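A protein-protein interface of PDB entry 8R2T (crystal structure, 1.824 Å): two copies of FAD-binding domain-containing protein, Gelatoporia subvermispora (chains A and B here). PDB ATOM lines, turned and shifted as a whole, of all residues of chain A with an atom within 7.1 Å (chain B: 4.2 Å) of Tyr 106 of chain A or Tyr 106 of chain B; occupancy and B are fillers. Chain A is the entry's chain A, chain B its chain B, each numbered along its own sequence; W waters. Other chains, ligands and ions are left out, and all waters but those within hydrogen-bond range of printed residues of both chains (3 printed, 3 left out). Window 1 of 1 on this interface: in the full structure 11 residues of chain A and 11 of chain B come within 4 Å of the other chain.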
ATOM      1  N   PRO A  90       9.103   5.023  21.991  1.00  0.00           N
ATOM      2  CA  PRO A  90       9.974   3.851  22.109  1.00  0.00           C
ATOM      3  C   PRO A  90      11.249   4.154  22.871  1.00  0.00           C
ATOM      4  O   PRO A  90      11.666   5.286  22.961  1.00  0.00           O
ATOM      5  CB  PRO A  90      10.282   3.487  20.643  1.00  0.00           C
ATOM      6  CG  PRO A  90      10.159   4.793  19.907  1.00  0.00           C
ATOM      7  CD  PRO A  90       9.007   5.491  20.590  1.00  0.00           C
ATOM      8  N   GLU A  91      11.849   3.121  23.445  1.00  0.00           N
ATOM      9  CA  GLU A  91      13.026   3.279  24.281  1.00  0.00           C
ATOM     10  C   GLU A  91      14.268   3.175  23.411  1.00  0.00           C
ATOM     11  O   GLU A  91      15.287   3.745  23.724  1.00  0.00           O
ATOM     12  CB  GLU A  91      13.160   2.162  25.306  1.00  0.00           C
ATOM     13  CG  GLU A  91      11.913   1.844  26.092  1.00  0.00           C
ATOM     14  CD  GLU A  91      11.583   2.856  27.148  1.00  0.00           C
ATOM     15  OE1 GLU A  91      10.537   2.645  27.772  1.00  0.00           O
ATOM     16  OE2 GLU A  91      12.367   3.840  27.337  1.00  0.00           O
ATOM     17  N   GLY A  92      14.205   2.308  22.390  1.00  0.00           N
ATOM     18  CA  GLY A  92      15.378   1.947  21.621  1.00  0.00           C
ATOM     19  C   GLY A  92      14.980   1.362  20.276  1.00  0.00           C
ATOM     20  O   GLY A  92      13.817   1.056  20.053  1.00  0.00           O
ATOM     21  N   MET A  93      15.963   1.305  19.388  1.00  0.00           N
ATOM     22  CA  MET A  93      15.872   0.670  18.088  1.00  0.00           C
ATOM     23  C   MET A  93      16.787  -0.547  18.113  1.00  0.00           C
ATOM     24  O   MET A  93      17.963  -0.416  18.458  1.00  0.00           O
ATOM     25  CB  MET A  93      16.277   1.669  17.008  1.00  0.00           C
ATOM     26  CG  MET A  93      16.270   1.156  15.594  1.00  0.00           C
ATOM     27  SD  MET A  93      16.477   2.557  14.408  1.00  0.00           S
ATOM     28  CE  MET A  93      15.124   3.647  14.825  1.00  0.00           C
ATOM     29  N   VAL A  94      16.209  -1.716  17.799  1.00  0.00           N
ATOM     30  CA  VAL A  94      16.872  -2.982  17.976  1.00  0.00           C
ATOM     31  C   VAL A  94      16.891  -3.705  16.637  1.00  0.00           C
ATOM     32  O   VAL A  94      15.834  -3.997  16.082  1.00  0.00           O
ATOM     33  CB  VAL A  94      16.165  -3.834  19.040  1.00  0.00           C
ATOM     34  CG1 VAL A  94      16.888  -5.157  19.261  1.00  0.00           C
ATOM     35  CG2 VAL A  94      16.003  -3.056  20.360  1.00  0.00           C
ATOM     36  N   PHE A  95      18.104  -4.061  16.188  1.00  0.00           N
ATOM     37  CA  PHE A  95      18.298  -4.798  14.954  1.00  0.00           C
ATOM     38  C   PHE A  95      18.692  -6.226  15.290  1.00  0.00           C
ATOM     39  O   PHE A  95      19.540  -6.432  16.158  1.00  0.00           O
ATOM     40  CB  PHE A  95      19.336  -4.114  14.074  1.00  0.00           C
ATOM     41  CG  PHE A  95      18.841  -2.845  13.436  1.00  0.00           C
ATOM     42  CD1 PHE A  95      17.942  -2.880  12.370  1.00  0.00           C
ATOM     43  CD2 PHE A  95      19.222  -1.610  13.936  1.00  0.00           C
ATOM     44  CE1 PHE A  95      17.489  -1.706  11.789  1.00  0.00           C
ATOM     45  CE2 PHE A  95      18.762  -0.439  13.359  1.00  0.00           C
ATOM     46  CZ  PHE A  95      17.898  -0.488  12.286  1.00  0.00           C
ATOM     47  N   VAL A 103      20.013 -10.238  18.816  1.00  0.00           N
ATOM     48  CA  VAL A 103      20.190  -8.804  18.717  1.00  0.00           C
ATOM     49  C   VAL A 103      21.612  -8.554  18.232  1.00  0.00           C
ATOM     50  O   VAL A 103      22.570  -9.044  18.847  1.00  0.00           O
ATOM     51  CB  VAL A 103      19.932  -8.091  20.059  1.00  0.00           C
ATOM     52  CG1 VAL A 103      20.258  -6.603  19.932  1.00  0.00           C
ATOM     53  CG2 VAL A 103      18.499  -8.245  20.570  1.00  0.00           C
ATOM     54  N   VAL A 104      21.752  -7.790  17.140  1.00  0.00           N
ATOM     55  CA  VAL A 104      23.071  -7.449  16.608  1.00  0.00           C
ATOM     56  C   VAL A 104      23.290  -5.944  16.739  1.00  0.00           C
ATOM     57  O   VAL A 104      24.435  -5.527  16.686  1.00  0.00           O
ATOM     58  CB  VAL A 104      23.300  -7.904  15.158  1.00  0.00           C
ATOM     59  CG1 VAL A 104      23.161  -9.404  14.973  1.00  0.00           C
ATOM     60  CG2 VAL A 104      22.360  -7.215  14.192  1.00  0.00           C
ATOM     61  N   GLY A 105      22.232  -5.125  16.944  1.00  0.00           N
ATOM     62  CA  GLY A 105      22.455  -3.707  17.190  1.00  0.00           C
ATOM     63  C   GLY A 105      21.411  -3.054  18.078  1.00  0.00           C
ATOM     64  O   GLY A 105      20.260  -3.457  18.042  1.00  0.00           O
ATOM     65  N   TYR A 106      21.832  -1.964  18.754  1.00  0.00           N
ATOM     66  CA  TYR A 106      20.947  -1.137  19.553  1.00  0.00           C
ATOM     67  C   TYR A 106      21.304   0.317  19.283  1.00  0.00           C
ATOM     68  O   TYR A 106      22.476   0.665  19.246  1.00  0.00           O
ATOM     69  CB  TYR A 106      21.073  -1.497  21.043  1.00  0.00           C
ATOM     70  CG  TYR A 106      20.104  -0.816  21.970  1.00  0.00           C
ATOM     71  CD1 TYR A 106      20.406   0.394  22.554  1.00  0.00           C
ATOM     72  CD2 TYR A 106      18.853  -1.344  22.221  1.00  0.00           C
ATOM     73  CE1 TYR A 106      19.496   1.068  23.346  1.00  0.00           C
ATOM     74  CE2 TYR A 106      17.941  -0.711  23.060  1.00  0.00           C
ATOM     75  CZ  TYR A 106      18.265   0.509  23.621  1.00  0.00           C
ATOM     76  OH  TYR A 106      17.385   1.165  24.442  1.00  0.00           O
ATOM     77  N   ALA A 107      20.287   1.156  19.088  1.00  0.00           N
ATOM     78  CA  ALA A 107      20.437   2.596  19.203  1.00  0.00           C
ATOM     79  C   ALA A 107      19.424   3.120  20.203  1.00  0.00           C
ATOM     80  O   ALA A 107      18.221   2.924  20.037  1.00  0.00           O
ATOM     81  CB  ALA A 107      20.244   3.283  17.870  1.00  0.00           C
ATOM     82  N   ARG A 108      19.927   3.819  21.213  1.00  0.00           N
ATOM     83  CA  ARG A 108      19.067   4.382  22.238  1.00  0.00           C
ATOM     84  C   ARG A 108      18.170   5.438  21.616  1.00  0.00           C
ATOM     85  O   ARG A 108      18.658   6.256  20.842  1.00  0.00           O
ATOM     86  CB  ARG A 108      19.906   5.024  23.325  1.00  0.00           C
ATOM     87  CG  ARG A 108      19.090   5.548  24.494  1.00  0.00           C
ATOM     88  CD  ARG A 108      18.300   4.442  25.169  1.00  0.00           C
ATOM     89  NE  ARG A 108      17.623   5.011  26.313  1.00  0.00           N
ATOM     90  CZ  ARG A 108      16.899   4.311  27.175  1.00  0.00           C
ATOM     91  NH1 ARG A 108      16.696   3.030  26.910  1.00  0.00           N
ATOM     92  NH2 ARG A 108      16.408   4.879  28.280  1.00  0.00           N
ATOM     93  N   LEU A 109      16.863   5.368  21.905  1.00  0.00           N
ATOM     94  CA  LEU A 109      15.966   6.443  21.525  1.00  0.00           C
ATOM     95  C   LEU A 109      15.663   7.211  22.810  1.00  0.00           C
ATOM     96  O   LEU A 109      16.593   7.628  23.498  1.00  0.00           O
ATOM     97  CB  LEU A 109      14.759   5.874  20.765  1.00  0.00           C
ATOM     98  CG  LEU A 109      15.098   5.051  19.514  1.00  0.00           C
ATOM     99  CD1 LEU A 109      13.862   4.410  18.948  1.00  0.00           C
ATOM    100  CD2 LEU A 109      15.772   5.882  18.442  1.00  0.00           C
ATOM    101  N   ALA A 110      14.395   7.425  23.154  1.00  0.00           N
ATOM    102  CA  ALA A 110      14.084   7.939  24.485  1.00  0.00           C
ATOM    103  C   ALA A 110      14.867   9.244  24.718  1.00  0.00           C
ATOM    104  O   ALA A 110      14.808  10.134  23.884  1.00  0.00           O
ATOM    105  CB  ALA A 110      14.362   6.834  25.514  1.00  0.00           C
ATOM    106  N   GLU A 111      15.571   9.375  25.860  1.00  0.00           N
ATOM    107  CA  GLU A 111      16.238  10.613  26.223  1.00  0.00           C
ATOM    108  C   GLU A 111      17.408  10.954  25.292  1.00  0.00           C
ATOM    109  O   GLU A 111      17.775  12.120  25.190  1.00  0.00           O
ATOM    110  CB  GLU A 111      16.704  10.587  27.678  1.00  0.00           C
ATOM    111  CG  GLU A 111      17.929   9.722  27.917  1.00  0.00           C
ATOM    112  CD  GLU A 111      17.696   8.247  27.686  1.00  0.00           C
ATOM    113  OE1 GLU A 111      16.583   7.764  28.015  1.00  0.00           O
ATOM    114  OE2 GLU A 111      18.650   7.581  27.225  1.00  0.00           O
ATOM    115  N   ARG A 112      17.983   9.952  24.611  1.00  0.00           N
ATOM    116  CA  ARG A 112      19.033  10.196  23.637  1.00  0.00           C
ATOM    117  C   ARG A 112      18.502  11.022  22.469  1.00  0.00           C
ATOM    118  O   ARG A 112      19.204  11.866  21.930  1.00  0.00           O
ATOM    119  CB  ARG A 112      19.589   8.866  23.152  1.00  0.00           C
ATOM    120  CG  ARG A 112      20.905   8.982  22.399  1.00  0.00           C
ATOM    121  CD  ARG A 112      22.122   9.356  23.245  1.00  0.00           C
ATOM    122  NE  ARG A 112      22.335   8.426  24.348  1.00  0.00           N
ATOM    123  CZ  ARG A 112      22.768   7.177  24.249  1.00  0.00           C
ATOM    124  NH1 ARG A 112      23.222   6.705  23.104  1.00  0.00           N
ATOM    125  NH2 ARG A 112      22.771   6.412  25.325  1.00  0.00           N
ATOM    126  N   GLU A 223       9.948  -0.902  21.570  1.00  0.00           N
ATOM    127  CA  GLU A 223      11.094  -0.626  20.723  1.00  0.00           C
ATOM    128  C   GLU A 223      10.701  -0.650  19.251  1.00  0.00           C
ATOM    129  O   GLU A 223       9.631  -1.125  18.867  1.00  0.00           O
ATOM    130  CB  GLU A 223      12.202  -1.638  20.991  1.00  0.00           C
ATOM    131  CG  GLU A 223      12.704  -1.631  22.411  1.00  0.00           C
ATOM    132  CD  GLU A 223      13.625  -2.784  22.768  1.00  0.00           C
ATOM    133  OE1 GLU A 223      14.617  -2.484  23.502  1.00  0.00           O
ATOM    134  OE2 GLU A 223      13.311  -3.989  22.373  1.00  0.00           O
ATOM    135  N   MET A 395      27.320  -3.047  14.141  1.00  0.00           N
ATOM    136  CA  MET A 395      26.105  -2.692  14.842  1.00  0.00           C
ATOM    137  C   MET A 395      26.238  -3.001  16.341  1.00  0.00           C
ATOM    138  O   MET A 395      25.774  -2.227  17.188  1.00  0.00           O
ATOM    139  CB  MET A 395      24.908  -3.413  14.224  1.00  0.00           C
ATOM    140  CG  MET A 395      24.413  -2.779  12.925  1.00  0.00           C
ATOM    141  SD  MET A 395      22.785  -3.432  12.529  1.00  0.00           S
ATOM    142  CE  MET A 395      22.327  -2.417  11.124  1.00  0.00           C
ATOM    143  N   ARG A 396      26.933  -4.086  16.684  1.00  0.00           N
ATOM    144  CA  ARG A 396      27.143  -4.436  18.085  1.00  0.00           C
ATOM    145  C   ARG A 396      27.921  -3.331  18.808  1.00  0.00           C
ATOM    146  O   ARG A 396      27.592  -2.931  19.909  1.00  0.00           O
ATOM    147  CB  ARG A 396      27.898  -5.761  18.179  1.00  0.00           C
ATOM    148  CG  ARG A 396      27.058  -6.990  17.847  1.00  0.00           C
ATOM    149  CD  ARG A 396      27.949  -8.225  17.778  1.00  0.00           C
ATOM    150  NE  ARG A 396      27.205  -9.352  17.256  1.00  0.00           N
ATOM    151  CZ  ARG A 396      27.440  -9.971  16.099  1.00  0.00           C
ATOM    152  NH1 ARG A 396      28.457  -9.637  15.338  1.00  0.00           N
ATOM    153  NH2 ARG A 396      26.649 -10.959  15.714  1.00  0.00           N
ATOM    154  N   LYS A 397      28.975  -2.831  18.173  1.00  0.00           N
ATOM    155  CA  LYS A 397      29.857  -1.846  18.778  1.00  0.00           C
ATOM    156  C   LYS A 397      29.357  -0.416  18.565  1.00  0.00           C
ATOM    157  O   LYS A 397      29.942   0.519  19.098  1.00  0.00           O
ATOM    158  CB  LYS A 397      31.274  -2.054  18.239  1.00  0.00           C
ATOM    159  CG  LYS A 397      31.510  -1.622  16.800  1.00  0.00           C
ATOM    160  CD  LYS A 397      32.867  -2.039  16.231  1.00  0.00           C
ATOM    161  CE  LYS A 397      34.008  -1.587  17.114  1.00  0.00           C
ATOM    162  NZ  LYS A 397      35.329  -1.672  16.440  1.00  0.00           N
ATOM    163  N   ALA A 398      28.257  -0.230  17.830  1.00  0.00           N
ATOM    164  CA  ALA A 398      27.732   1.095  17.492  1.00  0.00           C
ATOM    165  C   ALA A 398      28.819   1.943  16.836  1.00  0.00           C
ATOM    166  O   ALA A 398      29.157   3.002  17.345  1.00  0.00           O
ATOM    167  CB  ALA A 398      27.147   1.790  18.698  1.00  0.00           C
ATOM    168  N   ASN A 429      24.419   0.909  11.741  1.00  0.00           N
ATOM    169  CA  ASN A 429      23.199   1.417  12.331  1.00  0.00           C
ATOM    170  C   ASN A 429      23.258   2.943  12.386  1.00  0.00           C
ATOM    171  O   ASN A 429      23.825   3.517  13.297  1.00  0.00           O
ATOM    172  CB  ASN A 429      23.021   0.839  13.740  1.00  0.00           C
ATOM    173  CG  ASN A 429      21.756   1.284  14.422  1.00  0.00           C
ATOM    174  OD1 ASN A 429      21.066   2.182  13.924  1.00  0.00           O
ATOM    175  ND2 ASN A 429      21.483   0.686  15.575  1.00  0.00           N
ATOM    176  N   TRP A 431      21.306   5.121  13.229  1.00  0.00           N
ATOM    177  CA  TRP A 431      20.653   5.754  14.375  1.00  0.00           C
ATOM    178  C   TRP A 431      21.497   5.676  15.654  1.00  0.00           C
ATOM    179  O   TRP A 431      21.158   6.321  16.647  1.00  0.00           O
ATOM    180  CB  TRP A 431      19.264   5.184  14.605  1.00  0.00           C
ATOM    181  CG  TRP A 431      18.273   5.496  13.529  1.00  0.00           C
ATOM    182  CD1 TRP A 431      17.319   6.471  13.551  1.00  0.00           C
ATOM    183  CD2 TRP A 431      18.045   4.730  12.332  1.00  0.00           C
ATOM    184  NE1 TRP A 431      16.559   6.407  12.414  1.00  0.00           N
ATOM    185  CE2 TRP A 431      16.961   5.330  11.665  1.00  0.00           C
ATOM    186  CE3 TRP A 431      18.646   3.599  11.754  1.00  0.00           C
ATOM    187  CZ2 TRP A 431      16.474   4.832  10.458  1.00  0.00           C
ATOM    188  CZ3 TRP A 431      18.144   3.107  10.581  1.00  0.00           C
ATOM    189  CH2 TRP A 431      17.103   3.748   9.917  1.00  0.00           C
ATOM    190  N   ALA A 432      22.588   4.905  15.615  1.00  0.00           N
ATOM    191  CA  ALA A 432      23.548   4.849  16.710  1.00  0.00           C
ATOM    192  C   ALA A 432      24.735   5.752  16.453  1.00  0.00           C
ATOM    193  O   ALA A 432      25.603   5.836  17.310  1.00  0.00           O
ATOM    194  CB  ALA A 432      24.042   3.433  16.946  1.00  0.00           C
ATOM    195  N   GLU B  91      20.843  -5.592  30.269  1.00  0.00           N
ATOM    196  CA  GLU B  91      20.691  -5.029  28.943  1.00  0.00           C
ATOM    197  C   GLU B  91      21.384  -3.681  28.858  1.00  0.00           C
ATOM    198  O   GLU B  91      21.891  -3.330  27.813  1.00  0.00           O
ATOM    199  CB  GLU B  91      19.211  -4.762  28.616  1.00  0.00           C
ATOM    200  CG  GLU B  91      18.323  -5.991  28.701  1.00  0.00           C
ATOM    201  CD  GLU B  91      18.632  -7.020  27.640  1.00  0.00           C
ATOM    202  OE1 GLU B  91      18.175  -8.136  27.779  1.00  0.00           O
ATOM    203  OE2 GLU B  91      19.340  -6.693  26.664  1.00  0.00           O
ATOM    204  N   GLY B  92      21.317  -2.925  29.956  1.00  0.00           N
ATOM    205  CA  GLY B  92      21.757  -1.561  29.953  1.00  0.00           C
ATOM    206  C   GLY B  92      21.971  -1.050  31.370  1.00  0.00           C
ATOM    207  O   GLY B  92      21.588  -1.699  32.342  1.00  0.00           O
ATOM    208  N   MET B  93      22.554   0.148  31.419  1.00  0.00           N
ATOM    209  CA  MET B  93      22.816   0.859  32.643  1.00  0.00           C
ATOM    210  C   MET B  93      22.043   2.166  32.568  1.00  0.00           C
ATOM    211  O   MET B  93      22.185   2.884  31.595  1.00  0.00           O
ATOM    212  CB  MET B  93      24.330   1.067  32.796  1.00  0.00           C
ATOM    213  CG  MET B  93      24.762   1.923  33.972  1.00  0.00           C
ATOM    214  SD  MET B  93      26.564   1.854  34.229  1.00  0.00           S
ATOM    215  CE  MET B  93      26.868   0.085  34.277  1.00  0.00           C
ATOM    216  N   VAL B  94      21.227   2.451  33.599  1.00  0.00           N
ATOM    217  CA  VAL B  94      20.232   3.505  33.550  1.00  0.00           C
ATOM    218  C   VAL B  94      20.438   4.397  34.762  1.00  0.00           C
ATOM    219  O   VAL B  94      20.338   3.917  35.886  1.00  0.00           O
ATOM    220  CB  VAL B  94      18.801   2.930  33.541  1.00  0.00           C
ATOM    221  CG1 VAL B  94      17.743   4.026  33.472  1.00  0.00           C
ATOM    222  CG2 VAL B  94      18.615   1.898  32.426  1.00  0.00           C
ATOM    223  N   GLY B 105      20.203   9.162  31.872  1.00  0.00           N
ATOM    224  CA  GLY B 105      21.250   8.540  31.071  1.00  0.00           C
ATOM    225  C   GLY B 105      21.025   7.046  30.854  1.00  0.00           C
ATOM    226  O   GLY B 105      20.415   6.374  31.672  1.00  0.00           O
ATOM    227  N   TYR B 106      21.556   6.549  29.731  1.00  0.00           N
ATOM    228  CA  TYR B 106      21.577   5.143  29.368  1.00  0.00           C
ATOM    229  C   TYR B 106      22.943   4.810  28.792  1.00  0.00           C
ATOM    230  O   TYR B 106      23.500   5.575  28.016  1.00  0.00           O
ATOM    231  CB  TYR B 106      20.484   4.841  28.325  1.00  0.00           C
ATOM    232  CG  TYR B 106      20.308   3.381  27.983  1.00  0.00           C
ATOM    233  CD1 TYR B 106      19.513   2.560  28.757  1.00  0.00           C
ATOM    234  CD2 TYR B 106      21.013   2.799  26.923  1.00  0.00           C
ATOM    235  CE1 TYR B 106      19.395   1.215  28.469  1.00  0.00           C
ATOM    236  CE2 TYR B 106      20.886   1.465  26.607  1.00  0.00           C
ATOM    237  CZ  TYR B 106      20.062   0.671  27.377  1.00  0.00           C
ATOM    238  OH  TYR B 106      19.879  -0.657  27.071  1.00  0.00           O
ATOM    239  N   ALA B 107      23.475   3.662  29.173  1.00  0.00           N
ATOM    240  CA  ALA B 107      24.598   3.058  28.490  1.00  0.00           C
ATOM    241  C   ALA B 107      24.247   1.613  28.164  1.00  0.00           C
ATOM    242  O   ALA B 107      23.950   0.839  29.056  1.00  0.00           O
ATOM    243  CB  ALA B 107      25.846   3.096  29.369  1.00  0.00           C
ATOM    244  N   ARG B 108      24.310   1.254  26.880  1.00  0.00           N
ATOM    245  CA  ARG B 108      24.001  -0.088  26.449  1.00  0.00           C
ATOM    246  C   ARG B 108      25.027  -1.068  27.023  1.00  0.00           C
ATOM    247  O   ARG B 108      26.217  -0.780  26.972  1.00  0.00           O
ATOM    248  CB  ARG B 108      24.034  -0.135  24.921  1.00  0.00           C
ATOM    249  CG  ARG B 108      23.653  -1.482  24.334  1.00  0.00           C
ATOM    250  CD  ARG B 108      22.248  -1.851  24.748  1.00  0.00           C
ATOM    251  NE  ARG B 108      21.884  -3.095  24.121  1.00  0.00           N
ATOM    252  CZ  ARG B 108      20.670  -3.643  24.178  1.00  0.00           C
ATOM    253  NH1 ARG B 108      19.755  -3.164  25.010  1.00  0.00           N
ATOM    254  NH2 ARG B 108      20.399  -4.708  23.441  1.00  0.00           N
ATOM    255  N   GLU B 111      25.121  -6.639  23.927  1.00  0.00           N
ATOM    256  CA  GLU B 111      26.030  -6.864  22.804  1.00  0.00           C
ATOM    257  C   GLU B 111      27.075  -5.762  22.666  1.00  0.00           C
ATOM    258  O   GLU B 111      28.110  -6.036  22.093  1.00  0.00           O
ATOM    259  CB  GLU B 111      25.279  -7.006  21.472  1.00  0.00           C
ATOM    260  CG  GLU B 111      24.666  -5.720  20.922  1.00  0.00           C
ATOM    261  CD  GLU B 111      23.619  -5.093  21.815  1.00  0.00           C
ATOM    262  OE1 GLU B 111      22.844  -5.862  22.417  1.00  0.00           O
ATOM    263  OE2 GLU B 111      23.557  -3.833  21.860  1.00  0.00           O
ATOM    264  N   ARG B 112      26.807  -4.541  23.197  1.00  0.00           N
ATOM    265  CA  ARG B 112      27.778  -3.453  23.198  1.00  0.00           C
ATOM    266  C   ARG B 112      29.011  -3.862  24.006  1.00  0.00           C
ATOM    267  O   ARG B 112      30.133  -3.556  23.634  1.00  0.00           O
ATOM    268  CB  ARG B 112      27.176  -2.180  23.785  1.00  0.00           C
ATOM    269  CG  ARG B 112      27.960  -0.908  23.489  1.00  0.00           C
ATOM    270  CD  ARG B 112      27.946  -0.469  22.018  1.00  0.00           C
ATOM    271  NE  ARG B 112      26.633  -0.277  21.402  1.00  0.00           N
ATOM    272  CZ  ARG B 112      25.773   0.687  21.705  1.00  0.00           C
ATOM    273  NH1 ARG B 112      26.110   1.670  22.533  1.00  0.00           N
ATOM    274  NH2 ARG B 112      24.562   0.675  21.177  1.00  0.00           N
ATOM    275  N   GLU B 223      18.459  -4.362  34.342  1.00  0.00           N
ATOM    276  CA  GLU B 223      19.370  -3.245  34.158  1.00  0.00           C
ATOM    277  C   GLU B 223      20.142  -2.995  35.456  1.00  0.00           C
ATOM    278  O   GLU B 223      19.750  -3.424  36.546  1.00  0.00           O
ATOM    279  CB  GLU B 223      18.617  -1.978  33.727  1.00  0.00           C
ATOM    280  CG  GLU B 223      17.893  -2.146  32.392  1.00  0.00           C
ATOM    281  CD  GLU B 223      16.913  -1.037  32.026  1.00  0.00           C
ATOM    282  OE1 GLU B 223      16.903  -0.682  30.836  1.00  0.00           O
ATOM    283  OE2 GLU B 223      16.158  -0.524  32.939  1.00  0.00           O
ATOM    284  N   ASN B 429      28.353   9.959  31.984  1.00  0.00           N
ATOM    285  CA  ASN B 429      28.195   8.522  32.082  1.00  0.00           C
ATOM    286  C   ASN B 429      29.374   7.805  31.436  1.00  0.00           C
ATOM    287  O   ASN B 429      29.386   7.569  30.233  1.00  0.00           O
ATOM    288  CB  ASN B 429      26.881   8.096  31.434  1.00  0.00           C
ATOM    289  CG  ASN B 429      26.583   6.626  31.571  1.00  0.00           C
ATOM    290  OD1 ASN B 429      27.441   5.831  31.958  1.00  0.00           O
ATOM    291  ND2 ASN B 429      25.369   6.267  31.181  1.00  0.00           N
ATOM    292  N   ALA B 432      28.889   5.023  28.840  1.00  0.00           N
ATOM    293  CA  ALA B 432      28.383   5.364  27.515  1.00  0.00           C
ATOM    294  C   ALA B 432      29.484   5.957  26.626  1.00  0.00           C
ATOM    295  O   ALA B 432      29.219   6.283  25.479  1.00  0.00           O
ATOM    296  CB  ALA B 432      27.215   6.315  27.622  1.00  0.00           C
HETATM  297  O   HOH W   1      21.338   8.333  27.242  1.00  0.00           O
HETATM  298  O   HOH W   2      23.180   3.343  21.967  1.00  0.00           O
HETATM  299  O   HOH W   3      16.628  -3.687  24.388  1.00  0.00           O
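O of Tyr 106 of chain A lies within hydrogen-bond range of NH2 of Arg 112 of chain B, 2.8 Å away. O of Arg 396 of chain A is in hydrogen-bond range of NE of Arg 112 of chain B (3.2 Å). The guanidinium group (NH2) of Arg 112 of chain A sits at hydrogen-bond distance from the backbone carbonyl oxygen (O) of Tyr 106 of chain B, at 2.9 Å.
The side-chain hydroxyl (OH) of Tyr 106 of chain A sits at hydrogen-bond distance from the backbone carbonyl oxygen (O) of Glu 91 of chain A. The side-chain hydroxyl (OH) of Tyr 106 of chain A sits at hydrogen-bond distance from the guanidinium group (NH1) of Arg 108 of chain A, 3.2 Å away. OE1 of Glu 111 of chain B lies within salt-bridge range of NH2 of Arg 108 of chain B, 2.9 Å away. The guanidinium group (NH2) of Arg 108 of chain A lies within salt-bridge range of the side-chain carboxylate (OE1) of Glu 111 of chain A (2.9 Å).
Among the printed residues, merely in contact across the chains: Arg 108 of chain A with Tyr 106 of chain B, Ala 398 of chain A with Arg 112 of chain B, Tyr 106 of chain A with Arg 108 of chain B, Glu 111 of chain A with Tyr 106 of chain B, Tyr 106 of chain A with Glu 111 of chain B, Tyr 106 of chain A with Tyr 106 of chain B, Val 103 of chain A with Glu 111 of chain B, Lys 397 of chain A with Arg 112 of chain B, Arg 396 of chain A with Glu 111 of chain B and Val 103 of chain A with Arg 108 of chain B.
Of chain B, only Tyr 106, Arg 108, Glu 111 and Arg 112 come within 4 Å of Tyr 106 of chain A. Of chain A, only Tyr 106, Arg 108, Glu 111 and Arg 112 come within 4 Å of Tyr 106 of chain B. Of the printed residues of chain B, Arg 112 of chain A touches Tyr 106 (2.9 Å). Of the printed residues of chain A, Arg 108 of chain B touches Val 103 (3.99 Å) and Tyr 106 (3.5 Å). Ala 107 of chain A touches none of the printed residues of chain B. Leu 109 of chain A touches none of the printed residues of chain B. The nearest printed residue of chain B that does not touch Tyr 106 of chain A is Glu 91 of chain B (6.6 Å).
Of the 24 printed residues of chain A, 8 touch a printed residue of chain B. Printed residues of chain A that touch a printed residue of chain B: Val 103, Tyr 106, Arg 108, Glu 111, Arg 112, Arg 396, Lys 397 and Ala 398. Hydrophobic or aromatic side chains of chain A within 4 Å of the printed part of chain B: Val 103, Tyr 106 and Ala 398. Of the 13 printed residues of chain B, 4 touch a printed residue of chain A. Printed residues of chain B that touch a printed residue of chain A: Tyr 106, Arg 108, Glu 111 and Arg 112. Among the printed residues, no Asp or Glu carboxylate lies within 4 Å of a Lys or Arg side-chain nitrogen of the other chain.
Tyr 106 of chain A touches its own counterpart, Tyr 106 of chain B. Tyr 106 of chain A touches Arg 108 of chain B, and with the chains exchanged Arg 108 of chain A touches Tyr 106 of chain B. Tyr 106 of chain A touches Glu 111 of chain B, and with the chains exchanged Glu 111 of chain A touches Tyr 106 of chain B. Tyr 106 of chain A touches Arg 112 of chain B, and with the chains exchanged Arg 112 of chain A touches Tyr 106 of chain B. 13 positions are printed for both chains. Of the 13 pairs that touch across the chains among the printed residues, 7 have their exchanged pair printed and touching as well.
Water W3 lies within hydrogen-bond range of OE1 of Glu 223 of chain A (2.5 Å) and NH1 of Arg 108 of chain B (3.2 Å). Water W1 lies within hydrogen-bond range of the side-chain carboxylate (OE2) of Glu 111 of chain A (2.8 Å), the guanidinium group (NE) of Arg 112 of chain A (3.1 Å) and the backbone NH (N) of Tyr 106 of chain B (3.1 Å). Water W2 lies within hydrogen-bond range of NH2 of Arg 112 of chain B (3.1 Å) and N of Arg 108 of chain A (3.4 Å).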
